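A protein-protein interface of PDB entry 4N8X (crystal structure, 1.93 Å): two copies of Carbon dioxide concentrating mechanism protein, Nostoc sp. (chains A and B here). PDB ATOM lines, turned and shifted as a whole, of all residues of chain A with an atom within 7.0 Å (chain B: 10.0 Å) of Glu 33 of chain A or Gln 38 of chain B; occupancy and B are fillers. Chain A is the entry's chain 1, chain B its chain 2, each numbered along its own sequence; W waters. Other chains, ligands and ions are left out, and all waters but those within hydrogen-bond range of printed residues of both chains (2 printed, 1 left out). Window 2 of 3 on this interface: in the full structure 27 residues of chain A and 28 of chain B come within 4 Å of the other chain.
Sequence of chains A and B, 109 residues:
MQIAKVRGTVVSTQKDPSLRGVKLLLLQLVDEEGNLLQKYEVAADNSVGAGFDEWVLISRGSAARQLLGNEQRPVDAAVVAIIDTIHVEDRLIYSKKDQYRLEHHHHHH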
ATOM      1  N   VAL A  30      -6.405  10.531 -28.657  1.00  0.00           N
ATOM      2  CA  VAL A  30      -5.459  11.199 -27.746  1.00  0.00           C
ATOM      3  C   VAL A  30      -4.105  11.215 -28.451  1.00  0.00           C
ATOM      4  O   VAL A  30      -3.767  10.248 -29.167  1.00  0.00           O
ATOM      5  CB  VAL A  30      -5.390  10.442 -26.384  1.00  0.00           C
ATOM      6  CG1 VAL A  30      -4.266  10.968 -25.490  1.00  0.00           C
ATOM      7  CG2 VAL A  30      -6.748  10.542 -25.636  1.00  0.00           C
ATOM      8  N   ASP A  31      -3.346  12.295 -28.295  1.00  0.00           N
ATOM      9  CA  ASP A  31      -2.002  12.334 -28.862  1.00  0.00           C
ATOM     10  C   ASP A  31      -0.964  11.771 -27.882  1.00  0.00           C
ATOM     11  O   ASP A  31      -1.305  11.313 -26.789  1.00  0.00           O
ATOM     12  CB  ASP A  31      -1.597  13.737 -29.382  1.00  0.00           C
ATOM     13  CG  ASP A  31      -1.275  14.742 -28.279  1.00  0.00           C
ATOM     14  OD1 ASP A  31      -1.206  14.387 -27.073  1.00  0.00           O
ATOM     15  OD2 ASP A  31      -1.069  15.933 -28.618  1.00  0.00           O
ATOM     16  N   GLU A  32       0.300  11.812 -28.279  1.00  0.00           N
ATOM     17  CA  GLU A  32       1.346  11.120 -27.527  1.00  0.00           C
ATOM     18  C   GLU A  32       1.514  11.722 -26.138  1.00  0.00           C
ATOM     19  O   GLU A  32       1.824  11.002 -25.189  1.00  0.00           O
ATOM     20  CB  GLU A  32       2.670  11.200 -28.286  1.00  0.00           C
ATOM     21  CG  GLU A  32       3.748  10.281 -27.738  1.00  0.00           C
ATOM     22  CD  GLU A  32       4.552  10.932 -26.626  1.00  0.00           C
ATOM     23  OE1 GLU A  32       4.546  12.182 -26.545  1.00  0.00           O
ATOM     24  OE2 GLU A  32       5.188  10.197 -25.828  1.00  0.00           O
ATOM     25  N   GLU A  33       1.339  13.039 -26.028  1.00  0.00           N
ATOM     26  CA  GLU A  33       1.547  13.756 -24.750  1.00  0.00           C
ATOM     27  C   GLU A  33       0.302  13.682 -23.842  1.00  0.00           C
ATOM     28  O   GLU A  33       0.310  14.210 -22.734  1.00  0.00           O
ATOM     29  CB  GLU A  33       1.897  15.223 -24.996  1.00  0.00           C
ATOM     30  CG  GLU A  33       3.312  15.483 -25.589  1.00  0.00           C
ATOM     31  CD  GLU A  33       3.326  15.548 -27.125  1.00  0.00           C
ATOM     32  OE1 GLU A  33       4.423  15.672 -27.721  1.00  0.00           O
ATOM     33  OE2 GLU A  33       2.246  15.482 -27.737  1.00  0.00           O
ATOM     34  N   GLY A  34      -0.765  13.047 -24.319  1.00  0.00           N
ATOM     35  CA  GLY A  34      -1.969  12.869 -23.519  1.00  0.00           C
ATOM     36  C   GLY A  34      -3.011  13.966 -23.707  1.00  0.00           C
ATOM     37  O   GLY A  34      -3.948  14.099 -22.903  1.00  0.00           O
ATOM     38  N   ASN A  35      -2.856  14.768 -24.759  1.00  0.00           N
ATOM     39  CA  ASN A  35      -3.907  15.738 -25.106  1.00  0.00           C
ATOM     40  C   ASN A  35      -5.005  15.165 -25.983  1.00  0.00           C
ATOM     41  O   ASN A  35      -4.756  14.414 -26.935  1.00  0.00           O
ATOM     42  CB  ASN A  35      -3.333  16.992 -25.780  1.00  0.00           C
ATOM     43  CG  ASN A  35      -2.114  17.522 -25.092  1.00  0.00           C
ATOM     44  OD1 ASN A  35      -2.184  18.030 -23.971  1.00  0.00           O
ATOM     45  ND2 ASN A  35      -0.983  17.484 -25.796  1.00  0.00           N
ATOM     46  N   TRP A  55     -10.281   6.153 -20.759  1.00  0.00           N
ATOM     47  CA  TRP A  55      -9.263   5.969 -21.779  1.00  0.00           C
ATOM     48  C   TRP A  55      -9.098   4.485 -22.129  1.00  0.00           C
ATOM     49  O   TRP A  55      -9.038   3.609 -21.261  1.00  0.00           O
ATOM     50  CB  TRP A  55      -7.928   6.541 -21.282  1.00  0.00           C
ATOM     51  CG  TRP A  55      -7.889   8.063 -21.264  1.00  0.00           C
ATOM     52  CD1 TRP A  55      -8.948   8.912 -21.101  1.00  0.00           C
ATOM     53  CD2 TRP A  55      -6.726   8.894 -21.421  1.00  0.00           C
ATOM     54  NE1 TRP A  55      -8.512  10.238 -21.140  1.00  0.00           N
ATOM     55  CE2 TRP A  55      -7.159  10.247 -21.336  1.00  0.00           C
ATOM     56  CE3 TRP A  55      -5.366   8.628 -21.604  1.00  0.00           C
ATOM     57  CZ2 TRP A  55      -6.274  11.332 -21.438  1.00  0.00           C
ATOM     58  CZ3 TRP A  55      -4.479   9.726 -21.718  1.00  0.00           C
ATOM     59  CH2 TRP A  55      -4.949  11.051 -21.625  1.00  0.00           C
ATOM     60  N   ARG A  91       6.963   9.358 -13.906  1.00  0.00           N
ATOM     61  CA  ARG A  91       5.922  10.367 -13.720  1.00  0.00           C
ATOM     62  C   ARG A  91       4.680  10.035 -14.556  1.00  0.00           C
ATOM     63  O   ARG A  91       4.785   9.561 -15.688  1.00  0.00           O
ATOM     64  CB  ARG A  91       6.469  11.760 -14.057  1.00  0.00           C
ATOM     65  CG  ARG A  91       5.524  12.660 -14.853  1.00  0.00           C
ATOM     66  CD  ARG A  91       6.285  13.653 -15.735  1.00  0.00           C
ATOM     67  NE  ARG A  91       5.480  14.080 -16.882  1.00  0.00           N
ATOM     68  CZ  ARG A  91       5.984  14.446 -18.063  1.00  0.00           C
ATOM     69  NH1 ARG A  91       7.304  14.455 -18.252  1.00  0.00           N
ATOM     70  NH2 ARG A  91       5.170  14.806 -19.055  1.00  0.00           N
ATOM     71  N   ILE A  93       1.763  10.298 -16.884  1.00  0.00           N
ATOM     72  CA  ILE A  93       1.074  11.008 -17.950  1.00  0.00           C
ATOM     73  C   ILE A  93      -0.427  10.918 -17.680  1.00  0.00           C
ATOM     74  O   ILE A  93      -1.184  11.881 -17.901  1.00  0.00           O
ATOM     75  CB  ILE A  93       1.413  10.409 -19.342  1.00  0.00           C
ATOM     76  CG1 ILE A  93       2.540  11.194 -20.022  1.00  0.00           C
ATOM     77  CG2 ILE A  93       0.171  10.331 -20.245  1.00  0.00           C
ATOM     78  CD1 ILE A  93       2.811  12.574 -19.432  1.00  0.00           C
ATOM     79  N   ARG B   7       8.971   5.483 -24.675  1.00  0.00           N
ATOM     80  CA  ARG B   7       8.686   6.680 -23.920  1.00  0.00           C
ATOM     81  C   ARG B   7       7.887   6.416 -22.652  1.00  0.00           C
ATOM     82  O   ARG B   7       7.915   7.214 -21.721  1.00  0.00           O
ATOM     83  CB  ARG B   7       8.008   7.706 -24.829  1.00  0.00           C
ATOM     84  CG  ARG B   7       8.991   8.284 -25.837  1.00  0.00           C
ATOM     85  CD  ARG B   7       9.117   9.786 -25.741  1.00  0.00           C
ATOM     86  NE  ARG B   7       9.731  10.327 -24.542  1.00  0.00           N
ATOM     87  CZ  ARG B   7       9.469  11.554 -24.095  1.00  0.00           C
ATOM     88  NH1 ARG B   7      10.065  12.015 -23.004  1.00  0.00           N
ATOM     89  NH2 ARG B   7       8.590  12.317 -24.745  1.00  0.00           N
ATOM     90  N   LEU B  26       4.445   2.582 -24.621  1.00  0.00           N
ATOM     91  CA  LEU B  26       4.220   3.800 -25.399  1.00  0.00           C
ATOM     92  C   LEU B  26       5.493   4.165 -26.181  1.00  0.00           C
ATOM     93  O   LEU B  26       6.555   4.482 -25.600  1.00  0.00           O
ATOM     94  CB  LEU B  26       3.843   4.976 -24.494  1.00  0.00           C
ATOM     95  CG  LEU B  26       3.591   6.321 -25.184  1.00  0.00           C
ATOM     96  CD1 LEU B  26       2.343   6.250 -26.065  1.00  0.00           C
ATOM     97  CD2 LEU B  26       3.436   7.411 -24.137  1.00  0.00           C
ATOM     98  N   LEU B  27       5.354   4.126 -27.497  1.00  0.00           N
ATOM     99  CA  LEU B  27       6.445   4.305 -28.419  1.00  0.00           C
ATOM    100  C   LEU B  27       6.177   5.549 -29.247  1.00  0.00           C
ATOM    101  O   LEU B  27       5.117   5.675 -29.855  1.00  0.00           O
ATOM    102  CB  LEU B  27       6.507   3.103 -29.335  1.00  0.00           C
ATOM    103  CG  LEU B  27       6.768   1.782 -28.591  1.00  0.00           C
ATOM    104  CD1 LEU B  27       6.983   0.645 -29.574  1.00  0.00           C
ATOM    105  CD2 LEU B  27       7.974   1.931 -27.673  1.00  0.00           C
ATOM    106  N   GLN B  28       7.131   6.469 -29.252  1.00  0.00           N
ATOM    107  CA  GLN B  28       6.979   7.706 -30.011  1.00  0.00           C
ATOM    108  C   GLN B  28       7.924   7.666 -31.205  1.00  0.00           C
ATOM    109  O   GLN B  28       9.125   7.454 -31.051  1.00  0.00           O
ATOM    110  CB  GLN B  28       7.286   8.902 -29.131  1.00  0.00           C
ATOM    111  CG  GLN B  28       7.025  10.259 -29.810  1.00  0.00           C
ATOM    112  CD  GLN B  28       7.150  11.423 -28.839  1.00  0.00           C
ATOM    113  OE1 GLN B  28       7.594  11.250 -27.707  1.00  0.00           O
ATOM    114  NE2 GLN B  28       6.778  12.622 -29.283  1.00  0.00           N
ATOM    115  N   LEU B  29       7.386   7.869 -32.397  1.00  0.00           N
ATOM    116  CA  LEU B  29       8.188   7.732 -33.609  1.00  0.00           C
ATOM    117  C   LEU B  29       9.251   8.824 -33.672  1.00  0.00           C
ATOM    118  O   LEU B  29       9.105   9.887 -33.064  1.00  0.00           O
ATOM    119  CB  LEU B  29       7.289   7.747 -34.854  1.00  0.00           C
ATOM    120  CG  LEU B  29       6.659   6.374 -35.185  1.00  0.00           C
ATOM    121  CD1 LEU B  29       6.015   5.719 -33.988  1.00  0.00           C
ATOM    122  CD2 LEU B  29       5.622   6.485 -36.299  1.00  0.00           C
ATOM    123  N   VAL B  30      10.355   8.560 -34.357  1.00  0.00           N
ATOM    124  CA  VAL B  30      11.356   9.602 -34.512  1.00  0.00           C
ATOM    125  C   VAL B  30      11.653   9.733 -35.990  1.00  0.00           C
ATOM    126  O   VAL B  30      11.362   8.818 -36.775  1.00  0.00           O
ATOM    127  CB  VAL B  30      12.663   9.318 -33.711  1.00  0.00           C
ATOM    128  CG1 VAL B  30      12.357   9.107 -32.244  1.00  0.00           C
ATOM    129  CG2 VAL B  30      13.379   8.090 -34.267  1.00  0.00           C
ATOM    130  N   ASP B  31      12.227  10.870 -36.370  1.00  0.00           N
ATOM    131  CA  ASP B  31      12.633  11.072 -37.752  1.00  0.00           C
ATOM    132  C   ASP B  31      13.977  10.397 -37.918  1.00  0.00           C
ATOM    133  O   ASP B  31      14.393   9.635 -37.055  1.00  0.00           O
ATOM    134  CB  ASP B  31      12.709  12.569 -38.115  1.00  0.00           C
ATOM    135  CG  ASP B  31      13.724  13.343 -37.286  1.00  0.00           C
ATOM    136  OD1 ASP B  31      14.677  12.748 -36.716  1.00  0.00           O
ATOM    137  OD2 ASP B  31      13.575  14.585 -37.223  1.00  0.00           O
ATOM    138  N   ASN B  35      14.971  12.844 -33.782  1.00  0.00           N
ATOM    139  CA  ASN B  35      14.055  13.808 -33.183  1.00  0.00           C
ATOM    140  C   ASN B  35      12.676  13.184 -33.008  1.00  0.00           C
ATOM    141  O   ASN B  35      12.123  12.620 -33.950  1.00  0.00           O
ATOM    142  CB  ASN B  35      13.943  15.056 -34.053  1.00  0.00           C
ATOM    143  CG  ASN B  35      15.252  15.766 -34.213  1.00  0.00           C
ATOM    144  OD1 ASN B  35      15.656  16.083 -35.332  1.00  0.00           O
ATOM    145  ND2 ASN B  35      15.926  16.041 -33.094  1.00  0.00           N
ATOM    146  N   LEU B  36      12.113  13.276 -31.809  1.00  0.00           N
ATOM    147  CA  LEU B  36      10.772  12.756 -31.596  1.00  0.00           C
ATOM    148  C   LEU B  36       9.705  13.487 -32.435  1.00  0.00           C
ATOM    149  O   LEU B  36       9.721  14.721 -32.570  1.00  0.00           O
ATOM    150  CB  LEU B  36      10.414  12.786 -30.107  1.00  0.00           C
ATOM    151  CG  LEU B  36      11.414  12.050 -29.221  1.00  0.00           C
ATOM    152  CD1 LEU B  36      11.430  12.686 -27.844  1.00  0.00           C
ATOM    153  CD2 LEU B  36      11.067  10.546 -29.143  1.00  0.00           C
ATOM    154  N   LEU B  37       8.784  12.705 -32.995  1.00  0.00           N
ATOM    155  CA  LEU B  37       7.663  13.229 -33.776  1.00  0.00           C
ATOM    156  C   LEU B  37       6.346  13.176 -32.995  1.00  0.00           C
ATOM    157  O   LEU B  37       6.221  12.436 -32.000  1.00  0.00           O
ATOM    158  CB  LEU B  37       7.505  12.395 -35.051  1.00  0.00           C
ATOM    159  CG  LEU B  37       8.724  12.318 -35.952  1.00  0.00           C
ATOM    160  CD1 LEU B  37       8.507  11.233 -37.007  1.00  0.00           C
ATOM    161  CD2 LEU B  37       8.962  13.670 -36.595  1.00  0.00           C
ATOM    162  N   GLN B  38       5.352  13.930 -33.479  1.00  0.00           N
ATOM    163  CA  GLN B  38       3.974  13.843 -32.958  1.00  0.00           C
ATOM    164  C   GLN B  38       3.158  12.671 -33.516  1.00  0.00           C
ATOM    165  O   GLN B  38       2.056  12.880 -34.032  1.00  0.00           O
ATOM    166  CB  GLN B  38       3.212  15.117 -33.291  1.00  0.00           C
ATOM    167  CG  GLN B  38       3.742  16.300 -32.557  1.00  0.00           C
ATOM    168  CD  GLN B  38       3.839  16.024 -31.066  1.00  0.00           C
ATOM    169  OE1 GLN B  38       4.917  16.120 -30.478  1.00  0.00           O
ATOM    170  NE2 GLN B  38       2.704  15.675 -30.445  1.00  0.00           N
ATOM    171  N   LYS B  39       3.709  11.462 -33.457  1.00  0.00           N
ATOM    172  CA  LYS B  39       2.947  10.238 -33.722  1.00  0.00           C
ATOM    173  C   LYS B  39       3.519   9.167 -32.833  1.00  0.00           C
ATOM    174  O   LYS B  39       4.711   9.197 -32.486  1.00  0.00           O
ATOM    175  CB  LYS B  39       3.053   9.717 -35.162  1.00  0.00           C
ATOM    176  CG  LYS B  39       3.547  10.662 -36.185  1.00  0.00           C
ATOM    177  CD  LYS B  39       2.530  10.861 -37.286  1.00  0.00           C
ATOM    178  CE  LYS B  39       2.202   9.554 -37.987  1.00  0.00           C
ATOM    179  NZ  LYS B  39       3.367   8.957 -38.709  1.00  0.00           N
ATOM    180  N   TYR B  40       2.681   8.194 -32.499  1.00  0.00           N
ATOM    181  CA  TYR B  40       3.085   7.178 -31.535  1.00  0.00           C
ATOM    182  C   TYR B  40       2.313   5.908 -31.812  1.00  0.00           C
ATOM    183  O   TYR B  40       1.360   5.882 -32.615  1.00  0.00           O
ATOM    184  CB  TYR B  40       2.766   7.663 -30.119  1.00  0.00           C
ATOM    185  CG  TYR B  40       1.277   7.684 -29.839  1.00  0.00           C
ATOM    186  CD1 TYR B  40       0.510   8.795 -30.192  1.00  0.00           C
ATOM    187  CD2 TYR B  40       0.640   6.597 -29.232  1.00  0.00           C
ATOM    188  CE1 TYR B  40      -0.856   8.835 -29.955  1.00  0.00           C
ATOM    189  CE2 TYR B  40      -0.720   6.623 -28.989  1.00  0.00           C
ATOM    190  CZ  TYR B  40      -1.460   7.736 -29.343  1.00  0.00           C
ATOM    191  OH  TYR B  40      -2.810   7.759 -29.099  1.00  0.00           O
ATOM    192  N   GLU B  41       2.728   4.835 -31.158  1.00  0.00           N
ATOM    193  CA  GLU B  41       1.934   3.620 -31.134  1.00  0.00           C
ATOM    194  C   GLU B  41       2.071   3.124 -29.721  1.00  0.00           C
ATOM    195  O   GLU B  41       3.149   3.270 -29.105  1.00  0.00           O
ATOM    196  CB  GLU B  41       2.508   2.534 -32.064  1.00  0.00           C
ATOM    197  CG  GLU B  41       2.288   2.722 -33.560  1.00  0.00           C
ATOM    198  CD  GLU B  41       0.825   2.642 -33.962  1.00  0.00           C
ATOM    199  OE1 GLU B  41       0.476   3.083 -35.089  1.00  0.00           O
ATOM    200  OE2 GLU B  41       0.009   2.135 -33.158  1.00  0.00           O
ATOM    201  N   ARG B  60       3.771  -2.631 -37.939  1.00  0.00           N
ATOM    202  CA  ARG B  60       2.380  -2.224 -37.726  1.00  0.00           C
ATOM    203  C   ARG B  60       1.422  -3.091 -38.570  1.00  0.00           C
ATOM    204  O   ARG B  60       1.863  -3.773 -39.513  1.00  0.00           O
ATOM    205  CB  ARG B  60       2.189  -0.735 -38.119  1.00  0.00           C
ATOM    206  CG  ARG B  60       2.904   0.285 -37.204  1.00  0.00           C
ATOM    207  CD  ARG B  60       2.640   1.765 -37.633  1.00  0.00           C
ATOM    208  NE  ARG B  60       3.436   2.135 -38.794  1.00  0.00           N
ATOM    209  CZ  ARG B  60       3.425   3.339 -39.365  1.00  0.00           C
ATOM    210  NH1 ARG B  60       2.662   4.310 -38.886  1.00  0.00           N
ATOM    211  NH2 ARG B  60       4.182   3.570 -40.425  1.00  0.00           N
HETATM  212  O   HOH W   1       7.078  15.014 -27.289  1.00  0.00           O
HETATM  213  O   HOH W   2       0.578  12.725 -31.340  1.00  0.00           O
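Asp 31 of chain A touches just one residue of chain B: Tyr 40 (3.6 Å). Of the printed residues of chain B, Glu 32 of chain A touches Arg 7 (3.9 Å), Leu 26 (3.7 Å), Gln 28 (3.2 Å) and Tyr 40 (3.6 Å). Glu 33 of chain A touches just one residue of chain B: Gln 38. Gly 34 of chain A touches none of the printed residues of chain B. Of the printed residues of chain A, Leu 26 of chain B touches Glu 32 (3.7 Å). Gln 38 of chain B touches just one residue of chain A: Glu 33. Printed residues of chain A within 4 Å of Tyr 40 of chain B: Val 30, Asp 31 and Glu 32. The nearest residue of chain B that does not touch Glu 33 of chain A is Gln 28 of chain B (4.2 Å). The nearest printed residue of chain A that does not touch Gln 28 of chain B is Glu 33 of chain A (4.2 Å).
Among the printed residues, 7 pairs touch across the chains. Among the printed residues, no Asp or Glu carboxylate lies within 4 Å of a Lys or Arg side-chain nitrogen of the other chain.
Positions printed for both chains: 30, 31 and 35.
The side-chain carboxylate (OE2) of Glu 32 of chain A lies close to the side-chain amide oxygen (OE1) of Gln 28 of chain B. The side-chain hydroxyl of Tyr 40 of chain B is in hydrogen-bond range of the backbone carbonyl oxygen of Val 30 of chain A. NE2 of Gln 38 of chain B lies within hydrogen-bond range of OE2 of Glu 33 of chain A (2.8 Å).
OD1 of Asp 31 of chain A sits at hydrogen-bond distance from N of Asn 35 of chain A (2.9 Å). The backbone NH (N) of Arg 7 of chain B sits at hydrogen-bond distance from the backbone carbonyl oxygen (O) of Leu 26 of chain B. NE2 of Gln 28 of chain B sits at hydrogen-bond distance from O of Leu 37 of chain B. The side-chain carboxylate of Asp 31 of chain A sits at hydrogen-bond distance from the backbone NH of Gly 34 of chain A. The guanidinium group (NH2) of Arg 7 of chain B sits close to the side-chain amide oxygen (OE1) of Gln 28 of chain B (3.3 Å). The side-chain carboxylate of Asp 31 of chain A is in hydrogen-bond range of the backbone NH of Glu 33 of chain A (3.1 Å).
Asp 31 of chain A touches Tyr 40 of chain B (C to CE1, 3.6 Å). Glu 32 of chain A touches Arg 7 of chain B (OE2 to CB, 3.9 Å). Leu 26 of chain B touches Glu 32 of chain A. CD1 of Tyr 40 of chain B touches N of Glu 32 of chain A (3.6 Å).
Water W1 lies within hydrogen-bond range of the side-chain carboxylate (OE1) of Glu 33 of chain A and the side-chain amide nitrogen (NE2) of Gln 28 of chain B. Water W2 lies within hydrogen-bond range of the backbone carbonyl oxygen (O) of Gln 38 of chain B and the backbone NH (N) of Glu 32 of chain A.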
